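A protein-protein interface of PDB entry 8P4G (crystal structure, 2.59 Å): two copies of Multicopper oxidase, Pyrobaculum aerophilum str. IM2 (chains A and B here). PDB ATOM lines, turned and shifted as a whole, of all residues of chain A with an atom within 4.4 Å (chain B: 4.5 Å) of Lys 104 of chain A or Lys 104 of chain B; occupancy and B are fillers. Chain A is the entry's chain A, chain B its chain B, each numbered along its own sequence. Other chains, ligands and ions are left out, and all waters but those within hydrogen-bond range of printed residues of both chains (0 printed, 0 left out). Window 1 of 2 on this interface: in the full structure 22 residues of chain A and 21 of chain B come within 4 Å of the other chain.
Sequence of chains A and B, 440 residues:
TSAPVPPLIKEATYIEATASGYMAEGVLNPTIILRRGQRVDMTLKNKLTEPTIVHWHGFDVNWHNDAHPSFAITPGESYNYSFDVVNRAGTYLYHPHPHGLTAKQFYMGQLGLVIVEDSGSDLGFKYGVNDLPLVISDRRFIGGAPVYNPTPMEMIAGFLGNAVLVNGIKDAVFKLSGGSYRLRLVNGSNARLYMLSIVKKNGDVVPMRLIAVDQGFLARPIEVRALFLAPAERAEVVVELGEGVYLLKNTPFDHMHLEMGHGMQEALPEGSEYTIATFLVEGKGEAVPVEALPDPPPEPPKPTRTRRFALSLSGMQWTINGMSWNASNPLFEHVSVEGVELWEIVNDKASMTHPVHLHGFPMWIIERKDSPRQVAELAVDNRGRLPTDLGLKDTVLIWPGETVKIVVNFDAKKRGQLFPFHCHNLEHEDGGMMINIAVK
NZ of Lys 104 of chain B lies within salt-bridge range of OE2 of Glu 50 of chain A (2.7 Å).
The side-chain amino group (NZ) of Lys 104 of chain A is in salt-bridge range of the side-chain carboxylate (OE2) of Glu 50 of chain B, 3.1 Å away.
The side-chain carboxylate (OE1) of Glu 50 of chain B sits at hydrogen-bond distance from the side-chain amide nitrogen (NE2) of Gln 105 of chain B, at 2.5 Å.
OE1 of Glu 50 of chain A is in hydrogen-bond range of NE2 of Gln 105 of chain A (2.5 Å).
Met 108 of chain B touches Glu 50 of chain A (CE to OE2, 3.997 Å).
Leu 101 of chain A touches Tyr 148 of chain B.
Lys 104 of chain B touches Lys 104 of chain A.
Leu 101 of chain B touches Tyr 148 of chain A (CD2 to O, 3.4 Å).
Printed residues of chain B within 4 Å of Leu 101 of chain A: Tyr 148.
Lys 104 of chain A touches two residues of chain B.
Lys 104 of chain B touches just these residues of chain A: Glu 50 and Lys 104.
Of the printed residues of chain A, Met 108 of chain B touches Glu 50.
Printed residues of chain A within 4 Å of Tyr 148 of chain B: Leu 101.
The nearest printed residue of chain B that does not touch Lys 104 of chain A is Leu 101 of chain B (5.1 Å).
The nearest printed residue of chain A that does not touch Lys 104 of chain B is Leu 101 of chain A (4.5 Å).
Of the 10 printed residues of chain B, 5 touch a printed residue of chain A.
Printed residues of chain A that touch a printed residue of chain B: Glu 50, Leu 101, Lys 104 and Tyr 148.
Among the printed residues, 6 pairs touch across the chains.
Among the printed residues, Asp or Glu carboxylates within 4 Å of a Lys or Arg side-chain nitrogen of the other chain: Glu 50 of chain A with Lys 104 of chain B (2.7 Å) and Lys 104 of chain A with Glu 50 of chain B (3.1 Å).
Glu 50 of chain A touches Lys 104 of chain B, and with the chains exchanged Lys 104 of chain A touches Glu 50 of chain B.
Glu 50 of chain A touches Met 108 of chain B, but with the chains exchanged Met 108 of chain A does not touch Glu 50 of chain B (4.1 Å).
Leu 101 of chain A touches Tyr 148 of chain B, and with the chains exchanged Tyr 148 of chain A touches Leu 101 of chain B.
Lys 104 of chain A touches its own counterpart, Lys 104 of chain B.
Positions printed for both chains: 50, 101, 102, 103, 104, 105, 106, 107, 108 and 148.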
ATOM      1  N   GLU A  50      -8.378   1.069   7.853  1.00  0.00           N
ATOM      2  CA  GLU A  50      -7.854   2.391   7.552  1.00  0.00           C
ATOM      3  C   GLU A  50      -6.353   2.266   7.354  1.00  0.00           C
ATOM      4  O   GLU A  50      -5.759   1.249   7.732  1.00  0.00           O
ATOM      5  CB  GLU A  50      -8.181   3.385   8.675  1.00  0.00           C
ATOM      6  CG  GLU A  50      -7.737   2.948  10.058  1.00  0.00           C
ATOM      7  CD  GLU A  50      -8.012   4.002  11.111  1.00  0.00           C
ATOM      8  OE1 GLU A  50      -7.085   4.329  11.882  1.00  0.00           O
ATOM      9  OE2 GLU A  50      -9.152   4.510  11.166  1.00  0.00           O
ATOM     10  N   LEU A 101      -4.577   9.585  12.207  1.00  0.00           N
ATOM     11  CA  LEU A 101      -5.140   8.331  12.685  1.00  0.00           C
ATOM     12  C   LEU A 101      -4.261   7.650  13.721  1.00  0.00           C
ATOM     13  O   LEU A 101      -4.598   6.550  14.172  1.00  0.00           O
ATOM     14  CB  LEU A 101      -5.373   7.374  11.507  1.00  0.00           C
ATOM     15  CG  LEU A 101      -6.198   7.914  10.339  1.00  0.00           C
ATOM     16  CD1 LEU A 101      -6.214   6.918   9.191  1.00  0.00           C
ATOM     17  CD2 LEU A 101      -7.610   8.237  10.790  1.00  0.00           C
ATOM     18  N   THR A 102      -3.148   8.274  14.112  1.00  0.00           N
ATOM     19  CA  THR A 102      -2.175   7.606  14.968  1.00  0.00           C
ATOM     20  C   THR A 102      -2.696   7.448  16.391  1.00  0.00           C
ATOM     21  O   THR A 102      -2.518   6.390  17.005  1.00  0.00           O
ATOM     22  CB  THR A 102      -0.858   8.387  14.964  1.00  0.00           C
ATOM     23  OG1 THR A 102      -0.299   8.378  13.644  1.00  0.00           O
ATOM     24  CG2 THR A 102       0.137   7.771  15.933  1.00  0.00           C
ATOM     25  N   ALA A 103      -3.350   8.483  16.923  1.00  0.00           N
ATOM     26  CA  ALA A 103      -3.700   8.501  18.340  1.00  0.00           C
ATOM     27  C   ALA A 103      -4.613   7.338  18.712  1.00  0.00           C
ATOM     28  O   ALA A 103      -4.386   6.656  19.718  1.00  0.00           O
ATOM     29  CB  ALA A 103      -4.355   9.833  18.702  1.00  0.00           C
ATOM     30  N   LYS A 104      -5.651   7.089  17.908  1.00  0.00           N
ATOM     31  CA  LYS A 104      -6.601   6.039  18.264  1.00  0.00           C
ATOM     32  C   LYS A 104      -6.006   4.654  18.036  1.00  0.00           C
ATOM     33  O   LYS A 104      -6.242   3.735  18.830  1.00  0.00           O
ATOM     34  CB  LYS A 104      -7.903   6.209  17.484  1.00  0.00           C
ATOM     35  CG  LYS A 104      -9.007   5.267  17.940  1.00  0.00           C
ATOM     36  CD  LYS A 104     -10.379   5.797  17.564  1.00  0.00           C
ATOM     37  CE  LYS A 104     -11.463   4.776  17.859  1.00  0.00           C
ATOM     38  NZ  LYS A 104     -12.194   4.377  16.623  1.00  0.00           N
ATOM     39  N   GLN A 105      -5.232   4.479  16.961  1.00  0.00           N
ATOM     40  CA  GLN A 105      -4.568   3.198  16.743  1.00  0.00           C
ATOM     41  C   GLN A 105      -3.590   2.903  17.872  1.00  0.00           C
ATOM     42  O   GLN A 105      -3.518   1.773  18.371  1.00  0.00           O
ATOM     43  CB  GLN A 105      -3.846   3.198  15.393  1.00  0.00           C
ATOM     44  CG  GLN A 105      -4.761   3.332  14.181  1.00  0.00           C
ATOM     45  CD  GLN A 105      -3.998   3.336  12.871  1.00  0.00           C
ATOM     46  OE1 GLN A 105      -2.800   3.063  12.835  1.00  0.00           O
ATOM     47  NE2 GLN A 105      -4.689   3.652  11.787  1.00  0.00           N
ATOM     48  N   PHE A 106      -2.829   3.917  18.285  1.00  0.00           N
ATOM     49  CA  PHE A 106      -1.949   3.801  19.443  1.00  0.00           C
ATOM     50  C   PHE A 106      -2.746   3.502  20.707  1.00  0.00           C
ATOM     51  O   PHE A 106      -2.465   2.530  21.419  1.00  0.00           O
ATOM     52  CB  PHE A 106      -1.159   5.103  19.591  1.00  0.00           C
ATOM     53  CG  PHE A 106       0.014   5.027  20.530  1.00  0.00           C
ATOM     54  CD1 PHE A 106       1.305   5.082  20.033  1.00  0.00           C
ATOM     55  CD2 PHE A 106      -0.170   4.950  21.903  1.00  0.00           C
ATOM     56  CE1 PHE A 106       2.389   5.037  20.882  1.00  0.00           C
ATOM     57  CE2 PHE A 106       0.912   4.900  22.758  1.00  0.00           C
ATOM     58  CZ  PHE A 106       2.193   4.944  22.247  1.00  0.00           C
ATOM     59  N   TYR A 107      -3.750   4.335  20.996  1.00  0.00           N
ATOM     60  CA  TYR A 107      -4.508   4.220  22.240  1.00  0.00           C
ATOM     61  C   TYR A 107      -5.199   2.866  22.357  1.00  0.00           C
ATOM     62  O   TYR A 107      -5.288   2.300  23.453  1.00  0.00           O
ATOM     63  CB  TYR A 107      -5.524   5.361  22.322  1.00  0.00           C
ATOM     64  CG  TYR A 107      -6.464   5.336  23.509  1.00  0.00           C
ATOM     65  CD1 TYR A 107      -6.168   6.041  24.668  1.00  0.00           C
ATOM     66  CD2 TYR A 107      -7.659   4.635  23.460  1.00  0.00           C
ATOM     67  CE1 TYR A 107      -7.029   6.034  25.750  1.00  0.00           C
ATOM     68  CE2 TYR A 107      -8.524   4.620  24.535  1.00  0.00           C
ATOM     69  CZ  TYR A 107      -8.206   5.321  25.677  1.00  0.00           C
ATOM     70  OH  TYR A 107      -9.073   5.305  26.748  1.00  0.00           O
ATOM     71  N   MET A 108      -5.691   2.327  21.243  1.00  0.00           N
ATOM     72  CA  MET A 108      -6.472   1.098  21.262  1.00  0.00           C
ATOM     73  C   MET A 108      -5.619  -0.167  21.230  1.00  0.00           C
ATOM     74  O   MET A 108      -6.174  -1.265  21.118  1.00  0.00           O
ATOM     75  CB  MET A 108      -7.466   1.085  20.099  1.00  0.00           C
ATOM     76  CG  MET A 108      -8.640   2.033  20.288  1.00  0.00           C
ATOM     77  SD  MET A 108      -9.611   1.632  21.757  1.00  0.00           S
ATOM     78  CE  MET A 108     -11.057   2.662  21.509  1.00  0.00           C
ATOM     79  N   TYR A 148     -12.049   5.785  23.269  1.00  0.00           N
ATOM     80  CA  TYR A 148     -11.300   6.952  22.801  1.00  0.00           C
ATOM     81  C   TYR A 148     -12.284   7.872  22.083  1.00  0.00           C
ATOM     82  O   TYR A 148     -12.496   7.744  20.874  1.00  0.00           O
ATOM     83  CB  TYR A 148     -10.137   6.545  21.897  1.00  0.00           C
ATOM     84  CG  TYR A 148      -9.305   7.713  21.415  1.00  0.00           C
ATOM     85  CD1 TYR A 148      -8.345   8.290  22.238  1.00  0.00           C
ATOM     86  CD2 TYR A 148      -9.477   8.236  20.141  1.00  0.00           C
ATOM     87  CE1 TYR A 148      -7.584   9.357  21.805  1.00  0.00           C
ATOM     88  CE2 TYR A 148      -8.720   9.303  19.698  1.00  0.00           C
ATOM     89  CZ  TYR A 148      -7.774   9.859  20.535  1.00  0.00           C
ATOM     90  OH  TYR A 148      -7.020  10.924  20.097  1.00  0.00           O
ATOM     91  N   GLU B  50     -14.899  -1.428  20.510  1.00  0.00           N
ATOM     92  CA  GLU B  50     -15.368  -0.315  21.319  1.00  0.00           C
ATOM     93  C   GLU B  50     -16.872  -0.465  21.479  1.00  0.00           C
ATOM     94  O   GLU B  50     -17.505  -1.217  20.729  1.00  0.00           O
ATOM     95  CB  GLU B  50     -15.018   1.030  20.667  1.00  0.00           C
ATOM     96  CG  GLU B  50     -15.522   1.188  19.241  1.00  0.00           C
ATOM     97  CD  GLU B  50     -15.225   2.561  18.666  1.00  0.00           C
ATOM     98  OE1 GLU B  50     -16.162   3.209  18.155  1.00  0.00           O
ATOM     99  OE2 GLU B  50     -14.057   3.002  18.746  1.00  0.00           O
ATOM    100  N   LEU B 101     -18.491   8.212  19.909  1.00  0.00           N
ATOM    101  CA  LEU B 101     -17.964   7.255  18.948  1.00  0.00           C
ATOM    102  C   LEU B 101     -18.843   7.096  17.717  1.00  0.00           C
ATOM    103  O   LEU B 101     -18.526   6.269  16.854  1.00  0.00           O
ATOM    104  CB  LEU B 101     -17.779   5.880  19.604  1.00  0.00           C
ATOM    105  CG  LEU B 101     -16.962   5.795  20.890  1.00  0.00           C
ATOM    106  CD1 LEU B 101     -17.026   4.378  21.438  1.00  0.00           C
ATOM    107  CD2 LEU B 101     -15.526   6.223  20.648  1.00  0.00           C
ATOM    108  N   THR B 102     -19.932   7.859  17.610  1.00  0.00           N
ATOM    109  CA  THR B 102     -20.913   7.611  16.557  1.00  0.00           C
ATOM    110  C   THR B 102     -20.379   8.001  15.185  1.00  0.00           C
ATOM    111  O   THR B 102     -20.572   7.265  14.210  1.00  0.00           O
ATOM    112  CB  THR B 102     -22.207   8.366  16.860  1.00  0.00           C
ATOM    113  OG1 THR B 102     -22.784   7.858  18.069  1.00  0.00           O
ATOM    114  CG2 THR B 102     -23.204   8.199  15.724  1.00  0.00           C
ATOM    115  N   ALA B 103     -19.696   9.145  15.092  1.00  0.00           N
ATOM    116  CA  ALA B 103     -19.329   9.688  13.787  1.00  0.00           C
ATOM    117  C   ALA B 103     -18.444   8.728  13.001  1.00  0.00           C
ATOM    118  O   ALA B 103     -18.670   8.512  11.805  1.00  0.00           O
ATOM    119  CB  ALA B 103     -18.640  11.040  13.953  1.00  0.00           C
ATOM    120  N   LYS B 104     -17.434   8.140  13.647  1.00  0.00           N
ATOM    121  CA  LYS B 104     -16.517   7.277  12.910  1.00  0.00           C
ATOM    122  C   LYS B 104     -17.164   5.942  12.554  1.00  0.00           C
ATOM    123  O   LYS B 104     -16.946   5.418  11.456  1.00  0.00           O
ATOM    124  CB  LYS B 104     -15.233   7.050  13.707  1.00  0.00           C
ATOM    125  CG  LYS B 104     -14.182   6.284  12.919  1.00  0.00           C
ATOM    126  CD  LYS B 104     -12.779   6.492  13.454  1.00  0.00           C
ATOM    127  CE  LYS B 104     -11.800   5.565  12.747  1.00  0.00           C
ATOM    128  NZ  LYS B 104     -10.407   5.697  13.257  1.00  0.00           N
ATOM    129  N   GLN B 105     -17.959   5.374  13.464  1.00  0.00           N
ATOM    130  CA  GLN B 105     -18.660   4.131  13.149  1.00  0.00           C
ATOM    131  C   GLN B 105     -19.642   4.339  12.007  1.00  0.00           C
ATOM    132  O   GLN B 105     -19.742   3.507  11.098  1.00  0.00           O
ATOM    133  CB  GLN B 105     -19.384   3.600  14.387  1.00  0.00           C
ATOM    134  CG  GLN B 105     -18.471   3.201  15.533  1.00  0.00           C
ATOM    135  CD  GLN B 105     -19.245   2.691  16.727  1.00  0.00           C
ATOM    136  OE1 GLN B 105     -20.453   2.473  16.646  1.00  0.00           O
ATOM    137  NE2 GLN B 105     -18.554   2.496  17.843  1.00  0.00           N
ATOM    138  N   PHE B 106     -20.378   5.449  12.047  1.00  0.00           N
ATOM    139  CA  PHE B 106     -21.258   5.826  10.947  1.00  0.00           C
ATOM    140  C   PHE B 106     -20.462   6.011   9.660  1.00  0.00           C
ATOM    141  O   PHE B 106     -20.772   5.405   8.627  1.00  0.00           O
ATOM    142  CB  PHE B 106     -21.991   7.112  11.332  1.00  0.00           C
ATOM    143  CG  PHE B 106     -23.158   7.466  10.451  1.00  0.00           C
ATOM    144  CD1 PHE B 106     -24.449   7.397  10.945  1.00  0.00           C
ATOM    145  CD2 PHE B 106     -22.966   7.927   9.159  1.00  0.00           C
ATOM    146  CE1 PHE B 106     -25.526   7.743  10.157  1.00  0.00           C
ATOM    147  CE2 PHE B 106     -24.041   8.273   8.367  1.00  0.00           C
ATOM    148  CZ  PHE B 106     -25.322   8.185   8.869  1.00  0.00           C
ATOM    149  N   TYR B 107     -19.420   6.845   9.716  1.00  0.00           N
ATOM    150  CA  TYR B 107     -18.642   7.190   8.529  1.00  0.00           C
ATOM    151  C   TYR B 107     -18.001   5.961   7.897  1.00  0.00           C
ATOM    152  O   TYR B 107     -17.914   5.862   6.667  1.00  0.00           O
ATOM    153  CB  TYR B 107     -17.578   8.222   8.910  1.00  0.00           C
ATOM    154  CG  TYR B 107     -16.609   8.612   7.818  1.00  0.00           C
ATOM    155  CD1 TYR B 107     -16.835   9.734   7.033  1.00  0.00           C
ATOM    156  CD2 TYR B 107     -15.450   7.878   7.595  1.00  0.00           C
ATOM    157  CE1 TYR B 107     -15.945  10.104   6.043  1.00  0.00           C
ATOM    158  CE2 TYR B 107     -14.557   8.237   6.605  1.00  0.00           C
ATOM    159  CZ  TYR B 107     -14.808   9.352   5.833  1.00  0.00           C
ATOM    160  OH  TYR B 107     -13.918   9.716   4.846  1.00  0.00           O
ATOM    161  N   MET B 108     -17.549   5.014   8.714  1.00  0.00           N
ATOM    162  CA  MET B 108     -16.807   3.861   8.223  1.00  0.00           C
ATOM    163  C   MET B 108     -17.703   2.716   7.762  1.00  0.00           C
ATOM    164  O   MET B 108     -17.188   1.642   7.433  1.00  0.00           O
ATOM    165  CB  MET B 108     -15.832   3.364   9.293  1.00  0.00           C
ATOM    166  CG  MET B 108     -14.634   4.284   9.504  1.00  0.00           C
ATOM    167  SD  MET B 108     -13.625   4.499   8.024  1.00  0.00           S
ATOM    168  CE  MET B 108     -12.195   5.334   8.709  1.00  0.00           C
ATOM    169  N   TYR B 148     -11.102   8.849   8.269  1.00  0.00           N
ATOM    170  CA  TYR B 148     -11.810   9.773   9.151  1.00  0.00           C
ATOM    171  C   TYR B 148     -10.779  10.318  10.135  1.00  0.00           C
ATOM    172  O   TYR B 148     -10.565   9.754  11.211  1.00  0.00           O
ATOM    173  CB  TYR B 148     -12.976   9.085   9.866  1.00  0.00           C
ATOM    174  CG  TYR B 148     -13.771  10.008  10.760  1.00  0.00           C
ATOM    175  CD1 TYR B 148     -14.725  10.868  10.228  1.00  0.00           C
ATOM    176  CD2 TYR B 148     -13.573  10.022  12.137  1.00  0.00           C
ATOM    177  CE1 TYR B 148     -15.454  11.715  11.038  1.00  0.00           C
ATOM    178  CE2 TYR B 148     -14.300  10.865  12.957  1.00  0.00           C
ATOM    179  CZ  TYR B 148     -15.238  11.710  12.401  1.00  0.00           C
ATOM    180  OH  TYR B 148     -15.963  12.555  13.207  1.00  0.00           O
